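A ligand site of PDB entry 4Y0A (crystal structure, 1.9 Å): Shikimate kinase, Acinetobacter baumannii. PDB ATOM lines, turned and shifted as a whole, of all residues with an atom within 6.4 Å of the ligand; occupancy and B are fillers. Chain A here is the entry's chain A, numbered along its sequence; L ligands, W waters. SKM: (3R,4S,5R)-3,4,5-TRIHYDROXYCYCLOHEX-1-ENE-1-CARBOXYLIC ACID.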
ATOM      1  N   PRO A  16     -11.052  13.607  -6.538  1.00  0.00           N
ATOM      2  CA  PRO A  16     -11.131  12.953  -5.236  1.00  0.00           C
ATOM      3  C   PRO A  16     -12.559  12.538  -4.857  1.00  0.00           C
ATOM      4  O   PRO A  16     -13.494  12.898  -5.541  1.00  0.00           O
ATOM      5  CB  PRO A  16     -10.613  14.004  -4.265  1.00  0.00           C
ATOM      6  CG  PRO A  16     -11.072  15.312  -4.960  1.00  0.00           C
ATOM      7  CD  PRO A  16     -10.778  15.051  -6.418  1.00  0.00           C
ATOM      8  N   MET A  17     -12.641  11.680  -3.852  1.00  0.00           N
ATOM      9  CA  MET A  17     -13.894  11.412  -3.132  1.00  0.00           C
ATOM     10  C   MET A  17     -14.482  12.807  -2.833  1.00  0.00           C
ATOM     11  O   MET A  17     -13.760  13.683  -2.356  1.00  0.00           O
ATOM     12  CB  MET A  17     -13.630  10.655  -1.866  1.00  0.00           C
ATOM     13  CG  MET A  17     -13.227   9.150  -2.032  1.00  0.00           C
ATOM     14  SD  MET A  17     -12.704   8.426  -0.476  1.00  0.00           S
ATOM     15  CE  MET A  17     -10.968   8.939  -0.333  1.00  0.00           C
ATOM     16  N   LYS A  21     -18.327  13.657  -8.832  1.00  0.00           N
ATOM     17  CA  LYS A  21     -18.165  12.961 -10.117  1.00  0.00           C
ATOM     18  C   LYS A  21     -19.443  12.285 -10.603  1.00  0.00           C
ATOM     19  O   LYS A  21     -19.757  12.328 -11.819  1.00  0.00           O
ATOM     20  CB  LYS A  21     -17.053  11.894 -10.038  1.00  0.00           C
ATOM     21  CG  LYS A  21     -15.662  12.506  -9.814  1.00  0.00           C
ATOM     22  CD  LYS A  21     -14.512  11.425  -9.771  1.00  0.00           C
ATOM     23  CE  LYS A  21     -14.609  10.476  -8.546  1.00  0.00           C
ATOM     24  NZ  LYS A  21     -14.418  11.104  -7.273  1.00  0.00           N
ATOM     25  N   ASP A  40     -17.111   2.858  -9.639  1.00  0.00           N
ATOM     26  CA  ASP A  40     -17.236   2.280  -8.296  1.00  0.00           C
ATOM     27  C   ASP A  40     -18.473   1.368  -8.252  1.00  0.00           C
ATOM     28  O   ASP A  40     -18.457   0.218  -7.752  1.00  0.00           O
ATOM     29  CB  ASP A  40     -17.344   3.374  -7.209  1.00  0.00           C
ATOM     30  CG  ASP A  40     -15.999   3.975  -6.841  1.00  0.00           C
ATOM     31  OD1 ASP A  40     -14.936   3.471  -7.329  1.00  0.00           O
ATOM     32  OD2 ASP A  40     -15.999   4.970  -6.052  1.00  0.00           O
ATOM     33  N   ILE A  43     -18.033  -1.885 -10.229  1.00  0.00           N
ATOM     34  CA  ILE A  43     -17.219  -2.852  -9.515  1.00  0.00           C
ATOM     35  C   ILE A  43     -18.114  -3.599  -8.500  1.00  0.00           C
ATOM     36  O   ILE A  43     -18.081  -4.807  -8.406  1.00  0.00           O
ATOM     37  CB  ILE A  43     -16.009  -2.176  -8.811  1.00  0.00           C
ATOM     38  CG1 ILE A  43     -14.975  -1.746  -9.814  1.00  0.00           C
ATOM     39  CG2 ILE A  43     -15.375  -3.098  -7.737  1.00  0.00           C
ATOM     40  CD1 ILE A  43     -14.030  -0.687  -9.188  1.00  0.00           C
ATOM     41  N   ILE A  51     -17.697  -2.004  -1.735  1.00  0.00           N
ATOM     42  CA  ILE A  51     -16.255  -1.657  -1.755  1.00  0.00           C
ATOM     43  C   ILE A  51     -15.594  -1.814  -0.364  1.00  0.00           C
ATOM     44  O   ILE A  51     -14.469  -2.294  -0.287  1.00  0.00           O
ATOM     45  CB  ILE A  51     -16.075  -0.209  -2.347  1.00  0.00           C
ATOM     46  CG1 ILE A  51     -16.430  -0.259  -3.851  1.00  0.00           C
ATOM     47  CG2 ILE A  51     -14.624   0.273  -2.205  1.00  0.00           C
ATOM     48  CD1 ILE A  51     -16.307   1.067  -4.640  1.00  0.00           C
ATOM     49  N   PHE A  55     -12.332  -4.179   0.158  1.00  0.00           N
ATOM     50  CA  PHE A  55     -11.133  -3.749   0.850  1.00  0.00           C
ATOM     51  C   PHE A  55     -10.855  -4.674   2.060  1.00  0.00           C
ATOM     52  O   PHE A  55      -9.699  -5.026   2.325  1.00  0.00           O
ATOM     53  CB  PHE A  55     -11.240  -2.305   1.348  1.00  0.00           C
ATOM     54  CG  PHE A  55     -10.745  -1.258   0.351  1.00  0.00           C
ATOM     55  CD1 PHE A  55     -11.464  -0.955  -0.784  1.00  0.00           C
ATOM     56  CD2 PHE A  55      -9.563  -0.580   0.591  1.00  0.00           C
ATOM     57  CE1 PHE A  55     -11.020   0.006  -1.667  1.00  0.00           C
ATOM     58  CE2 PHE A  55      -9.102   0.384  -0.278  1.00  0.00           C
ATOM     59  CZ  PHE A  55      -9.841   0.700  -1.384  1.00  0.00           C
ATOM     60  N   GLU A  60      -6.673  -3.396  -0.430  1.00  0.00           N
ATOM     61  CA  GLU A  60      -6.651  -2.352  -1.460  1.00  0.00           C
ATOM     62  C   GLU A  60      -6.090  -2.917  -2.789  1.00  0.00           C
ATOM     63  O   GLU A  60      -6.585  -2.596  -3.860  1.00  0.00           O
ATOM     64  CB  GLU A  60      -5.839  -1.160  -0.996  1.00  0.00           C
ATOM     65  CG  GLU A  60      -5.949   0.010  -2.033  1.00  0.00           C
ATOM     66  CD  GLU A  60      -5.416   1.369  -1.517  1.00  0.00           C
ATOM     67  OE1 GLU A  60      -5.076   1.485  -0.326  1.00  0.00           O
ATOM     68  OE2 GLU A  60      -5.302   2.311  -2.306  1.00  0.00           O
ATOM     69  N   PHE A  63      -8.937  -4.585  -4.530  1.00  0.00           N
ATOM     70  CA  PHE A  63      -9.749  -3.547  -5.168  1.00  0.00           C
ATOM     71  C   PHE A  63      -9.116  -2.980  -6.447  1.00  0.00           C
ATOM     72  O   PHE A  63      -9.798  -2.840  -7.462  1.00  0.00           O
ATOM     73  CB  PHE A  63     -10.044  -2.384  -4.187  1.00  0.00           C
ATOM     74  CG  PHE A  63     -10.899  -1.294  -4.804  1.00  0.00           C
ATOM     75  CD1 PHE A  63     -12.221  -1.511  -4.968  1.00  0.00           C
ATOM     76  CD2 PHE A  63     -10.333  -0.123  -5.322  1.00  0.00           C
ATOM     77  CE1 PHE A  63     -13.047  -0.544  -5.611  1.00  0.00           C
ATOM     78  CE2 PHE A  63     -11.131   0.853  -5.902  1.00  0.00           C
ATOM     79  CZ  PHE A  63     -12.480   0.634  -6.076  1.00  0.00           C
ATOM     80  N   ARG A  64      -7.815  -2.651  -6.413  1.00  0.00           N
ATOM     81  CA  ARG A  64      -7.163  -2.083  -7.623  1.00  0.00           C
ATOM     82  C   ARG A  64      -7.160  -3.044  -8.806  1.00  0.00           C
ATOM     83  O   ARG A  64      -7.328  -2.631  -9.960  1.00  0.00           O
ATOM     84  CB  ARG A  64      -5.726  -1.641  -7.336  1.00  0.00           C
ATOM     85  CG  ARG A  64      -5.589  -0.510  -6.265  1.00  0.00           C
ATOM     86  CD  ARG A  64      -6.264   0.866  -6.709  1.00  0.00           C
ATOM     87  NE  ARG A  64      -6.353   1.723  -5.516  1.00  0.00           N
ATOM     88  CZ  ARG A  64      -7.270   2.676  -5.320  1.00  0.00           C
ATOM     89  NH1 ARG A  64      -8.168   2.960  -6.262  1.00  0.00           N
ATOM     90  NH2 ARG A  64      -7.285   3.321  -4.146  1.00  0.00           N
ATOM     91  N   GLU A  67     -10.654  -2.964 -10.103  1.00  0.00           N
ATOM     92  CA  GLU A  67     -10.914  -1.648 -10.721  1.00  0.00           C
ATOM     93  C   GLU A  67     -10.247  -1.538 -12.095  1.00  0.00           C
ATOM     94  O   GLU A  67     -10.839  -1.009 -13.025  1.00  0.00           O
ATOM     95  CB  GLU A  67     -10.403  -0.539  -9.768  1.00  0.00           C
ATOM     96  CG  GLU A  67     -10.441   0.854 -10.331  1.00  0.00           C
ATOM     97  CD  GLU A  67      -9.949   1.873  -9.365  1.00  0.00           C
ATOM     98  OE1 GLU A  67      -8.807   1.760  -8.847  1.00  0.00           O
ATOM     99  OE2 GLU A  67     -10.739   2.784  -9.076  1.00  0.00           O
ATOM    100  N   THR A  84     -15.046   8.014 -12.640  1.00  0.00           N
ATOM    101  CA  THR A  84     -14.014   7.067 -12.202  1.00  0.00           C
ATOM    102  C   THR A  84     -13.905   7.079 -10.683  1.00  0.00           C
ATOM    103  O   THR A  84     -14.365   7.967 -10.015  1.00  0.00           O
ATOM    104  CB  THR A  84     -12.622   7.391 -12.782  1.00  0.00           C
ATOM    105  OG1 THR A  84     -12.194   8.658 -12.249  1.00  0.00           O
ATOM    106  CG2 THR A  84     -12.696   7.461 -14.298  1.00  0.00           C
ATOM    107  N   GLY A  85     -13.240   6.086 -10.108  1.00  0.00           N
ATOM    108  CA  GLY A  85     -13.050   6.109  -8.681  1.00  0.00           C
ATOM    109  C   GLY A  85     -11.962   7.100  -8.273  1.00  0.00           C
ATOM    110  O   GLY A  85     -11.118   7.461  -9.082  1.00  0.00           O
ATOM    111  N   GLY A  86     -12.028   7.608  -7.055  1.00  0.00           N
ATOM    112  CA  GLY A  86     -11.104   8.630  -6.602  1.00  0.00           C
ATOM    113  C   GLY A  86      -9.612   8.258  -6.715  1.00  0.00           C
ATOM    114  O   GLY A  86      -8.783   9.124  -6.891  1.00  0.00           O
ATOM    115  N   GLY A  87      -9.277   6.973  -6.600  1.00  0.00           N
ATOM    116  CA  GLY A  87      -7.898   6.548  -6.621  1.00  0.00           C
ATOM    117  C   GLY A  87      -7.552   5.849  -7.910  1.00  0.00           C
ATOM    118  O   GLY A  87      -6.497   5.218  -8.009  1.00  0.00           O
ATOM    119  N   ALA A  88      -8.418   5.946  -8.892  1.00  0.00           N
ATOM    120  CA  ALA A  88      -8.179   5.216 -10.150  1.00  0.00           C
ATOM    121  C   ALA A  88      -6.869   5.618 -10.796  1.00  0.00           C
ATOM    122  O   ALA A  88      -6.193   4.768 -11.399  1.00  0.00           O
ATOM    123  CB  ALA A  88      -9.288   5.453 -11.146  1.00  0.00           C
ATOM    124  N   THR A  90      -4.121   6.325  -9.451  1.00  0.00           N
ATOM    125  CA  THR A  90      -2.917   5.868  -8.749  1.00  0.00           C
ATOM    126  C   THR A  90      -2.187   4.754  -9.510  1.00  0.00           C
ATOM    127  O   THR A  90      -1.008   4.484  -9.248  1.00  0.00           O
ATOM    128  CB  THR A  90      -3.227   5.336  -7.309  1.00  0.00           C
ATOM    129  OG1 THR A  90      -4.138   4.212  -7.354  1.00  0.00           O
ATOM    130  CG2 THR A  90      -3.805   6.461  -6.374  1.00  0.00           C
ATOM    131  N   ASN A 123     -19.168   4.132   3.381  1.00  0.00           N
ATOM    132  CA  ASN A 123     -18.802   3.404   2.165  1.00  0.00           C
ATOM    133  C   ASN A 123     -17.435   3.796   1.574  1.00  0.00           C
ATOM    134  O   ASN A 123     -17.077   3.230   0.579  1.00  0.00           O
ATOM    135  CB  ASN A 123     -19.851   3.546   1.059  1.00  0.00           C
ATOM    136  CG  ASN A 123     -19.914   2.271   0.166  1.00  0.00           C
ATOM    137  OD1 ASN A 123     -20.056   1.163   0.652  1.00  0.00           O
ATOM    138  ND2 ASN A 123     -19.810   2.452  -1.126  1.00  0.00           N
ATOM    139  N   ARG A 124     -16.690   4.715   2.200  1.00  0.00           N
ATOM    140  CA  ARG A 124     -15.365   5.150   1.709  1.00  0.00           C
ATOM    141  C   ARG A 124     -14.298   4.534   2.608  1.00  0.00           C
ATOM    142  O   ARG A 124     -13.985   5.110   3.637  1.00  0.00           O
ATOM    143  CB  ARG A 124     -15.253   6.695   1.729  1.00  0.00           C
ATOM    144  CG  ARG A 124     -16.395   7.466   1.148  1.00  0.00           C
ATOM    145  CD  ARG A 124     -16.554   7.370  -0.304  1.00  0.00           C
ATOM    146  NE  ARG A 124     -17.423   8.488  -0.730  1.00  0.00           N
ATOM    147  CZ  ARG A 124     -17.471   8.994  -1.963  1.00  0.00           C
ATOM    148  NH1 ARG A 124     -16.710   8.482  -2.914  1.00  0.00           N
ATOM    149  NH2 ARG A 124     -18.287  10.038  -2.214  1.00  0.00           N
ATOM    150  N   PRO A 125     -13.771   3.351   2.258  1.00  0.00           N
ATOM    151  CA  PRO A 125     -12.910   2.667   3.237  1.00  0.00           C
ATOM    152  C   PRO A 125     -11.726   3.511   3.648  1.00  0.00           C
ATOM    153  O   PRO A 125     -11.336   3.449   4.790  1.00  0.00           O
ATOM    154  CB  PRO A 125     -12.438   1.414   2.491  1.00  0.00           C
ATOM    155  CG  PRO A 125     -13.514   1.137   1.498  1.00  0.00           C
ATOM    156  CD  PRO A 125     -14.007   2.532   1.069  1.00  0.00           C
ATOM    157  N   LEU A 126     -11.172   4.332   2.750  1.00  0.00           N
ATOM    158  CA  LEU A 126      -9.934   5.004   3.143  1.00  0.00           C
ATOM    159  C   LEU A 126     -10.223   6.092   4.167  1.00  0.00           C
ATOM    160  O   LEU A 126      -9.315   6.575   4.814  1.00  0.00           O
ATOM    161  CB  LEU A 126      -9.225   5.605   1.936  1.00  0.00           C
ATOM    162  CG  LEU A 126      -8.744   4.624   0.898  1.00  0.00           C
ATOM    163  CD1 LEU A 126      -8.070   5.427  -0.227  1.00  0.00           C
ATOM    164  CD2 LEU A 126      -7.770   3.624   1.481  1.00  0.00           C
ATOM    165  N   LEU A 139      -3.852  12.501   0.626  1.00  0.00           N
ATOM    166  CA  LEU A 139      -4.193  11.873  -0.614  1.00  0.00           C
ATOM    167  C   LEU A 139      -4.110  12.854  -1.749  1.00  0.00           C
ATOM    168  O   LEU A 139      -3.607  12.535  -2.827  1.00  0.00           O
ATOM    169  CB  LEU A 139      -5.594  11.283  -0.539  1.00  0.00           C
ATOM    170  CG  LEU A 139      -5.788   9.969   0.214  1.00  0.00           C
ATOM    171  CD1 LEU A 139      -7.264   9.607   0.207  1.00  0.00           C
ATOM    172  CD2 LEU A 139      -4.991   8.793  -0.368  1.00  0.00           C
ATOM    173  N   ARG A 143      -2.095  12.786  -5.195  1.00  0.00           N
ATOM    174  CA  ARG A 143      -2.893  12.503  -6.377  1.00  0.00           C
ATOM    175  C   ARG A 143      -3.199  13.707  -7.266  1.00  0.00           C
ATOM    176  O   ARG A 143      -3.411  13.572  -8.488  1.00  0.00           O
ATOM    177  CB  ARG A 143      -4.195  11.827  -5.945  1.00  0.00           C
ATOM    178  CG  ARG A 143      -3.904  10.519  -5.209  1.00  0.00           C
ATOM    179  CD  ARG A 143      -5.161   9.993  -4.733  1.00  0.00           C
ATOM    180  NE  ARG A 143      -5.019   8.656  -4.159  1.00  0.00           N
ATOM    181  CZ  ARG A 143      -6.094   7.971  -3.782  1.00  0.00           C
ATOM    182  NH1 ARG A 143      -7.290   8.548  -3.877  1.00  0.00           N
ATOM    183  NH2 ARG A 143      -5.983   6.740  -3.310  1.00  0.00           N
ATOM    184  N   TYR A 147      -3.994  13.585 -11.162  1.00  0.00           N
ATOM    185  CA  TYR A 147      -5.268  14.006 -11.750  1.00  0.00           C
ATOM    186  C   TYR A 147      -4.977  14.972 -12.909  1.00  0.00           C
ATOM    187  O   TYR A 147      -5.528  14.865 -13.986  1.00  0.00           O
ATOM    188  CB  TYR A 147      -6.160  14.712 -10.762  1.00  0.00           C
ATOM    189  CG  TYR A 147      -6.725  13.866  -9.612  1.00  0.00           C
ATOM    190  CD1 TYR A 147      -7.398  12.651  -9.857  1.00  0.00           C
ATOM    191  CD2 TYR A 147      -6.616  14.301  -8.316  1.00  0.00           C
ATOM    192  CE1 TYR A 147      -7.927  11.903  -8.805  1.00  0.00           C
ATOM    193  CE2 TYR A 147      -7.144  13.543  -7.262  1.00  0.00           C
ATOM    194  CZ  TYR A 147      -7.792  12.370  -7.503  1.00  0.00           C
ATOM    195  OH  TYR A 147      -8.254  11.653  -6.398  1.00  0.00           O
HETATM  196  O12 SKM L   1     -12.937   3.910  -5.610  1.00  0.00           O
HETATM  197  C8  SKM L   1     -13.375   4.090  -4.251  1.00  0.00           C
HETATM  198  C6  SKM L   1     -12.540   3.504  -3.287  1.00  0.00           C
HETATM  199  O7  SKM L   1     -13.060   3.729  -1.944  1.00  0.00           O
HETATM  200  C5  SKM L   1     -11.047   4.069  -3.277  1.00  0.00           C
HETATM  201  C4  SKM L   1     -10.921   5.549  -3.496  1.00  0.00           C
HETATM  202  C1  SKM L   1      -9.649   6.260  -3.400  1.00  0.00           C
HETATM  203  O2  SKM L   1      -8.601   5.566  -3.586  1.00  0.00           O
HETATM  204  O3  SKM L   1      -9.617   7.524  -3.200  1.00  0.00           O
HETATM  205  C10 SKM L   1     -12.176   6.354  -3.812  1.00  0.00           C
HETATM  206  C9  SKM L   1     -13.449   5.763  -3.993  1.00  0.00           C
HETATM  207  O11 SKM L   1     -14.108   6.401  -5.131  1.00  0.00           O
HETATM  208  O   HOH W   1     -10.546   4.381  -6.833  1.00  0.00           O
HETATM  209  O   HOH W   2     -12.249   5.217   0.219  1.00  0.00           O
HETATM  210  O   HOH W   3     -10.126  10.185  -3.263  1.00  0.00           O
HETATM  211  O   HOH W   4     -16.908   5.552  -3.400  1.00  0.00           O
HETATM  212  O   HOH W   5     -14.908   9.021  -5.534  1.00  0.00           O
HETATM  213  O   HOH W   6     -15.698   3.777  -1.812  1.00  0.00           O
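O2 of the ligand is in salt-bridge range of NH2 of Arg 64 (2.7 Å).
The side-chain carboxylate (OD2) of Asp 40 is in hydrogen-bond range of an oxygen (O11) of the ligand, at 2.5 Å.
The backbone NH of Gly 86 lies within hydrogen-bond range of an oxygen (O11) of the ligand (3.1 Å).
O2 of the ligand lies close to N of Gly 87 (3.4 Å).
NH1 of Arg 143 lies within salt-bridge range of O3 of the ligand (2.6 Å).
NH1 of Arg 64 sits at hydrogen-bond distance from O of Gly 87 (3.3 Å).
The side-chain carboxylate (OE2) of Glu 60 is in salt-bridge range of the guanidinium group (NH2) of Arg 64.
The backbone carbonyl oxygen (O) of Gly 87 sits at hydrogen-bond distance from the side-chain hydroxyl (OG1) of Thr 90 (2.6 Å).
O of Gly 86 lies within hydrogen-bond range of OH of Tyr 147 (2.6 Å).
O of Gly 86 is in hydrogen-bond range of NH1 of Arg 143.
The side-chain carboxylate (OE1) of Glu 67 lies within salt-bridge range of the guanidinium group (NH1) of Arg 64, at 2.9 Å.
Met 17 touches the ligand (CE to O3, 3.5 Å).
CG2 of Ile 51 touches O7 of the ligand (3.8 Å).
CZ of Phe 63 touches O12 of the ligand, 3.3 Å away.
CA of Gly 85 touches O11 of the ligand, 3.7 Å away.
Pro 125 touches the ligand (CD to O7, 3.4 Å).
Leu 126 touches the ligand.
Hydrophobic or aromatic side chains that line the ligand: Met 17, Ile 51, Phe 63, Pro 125 and Leu 126.
The nearest printed residue that does not touch the ligand is Arg 124 (4.002 Å).
Water W6 bridges O7 of the ligand (2.6 Å) and O of Asn 123 (2.8 Å).
Water W3 lies within hydrogen-bond range of an oxygen (O3) of the ligand (2.7 Å), the backbone NH (N) of Met 17 (3.0 Å) and the guanidinium group (NH1) of Arg 143 (3.3 Å).
Water W2 lies within hydrogen-bond range of O7 of the ligand, N of Leu 126 and SD of Met 17.
Water W5 lies within hydrogen-bond range of the side-chain amino group (NZ) of Lys 21, an oxygen (O11) of the ligand and the guanidinium group (NH1) of Arg 124.
Water W4 lies within hydrogen-bond range of the side-chain carboxylate of Asp 40 (2.9 Å), the guanidinium group of Arg 124 (3.0 Å) and an oxygen (O11) of the ligand (3.4 Å).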
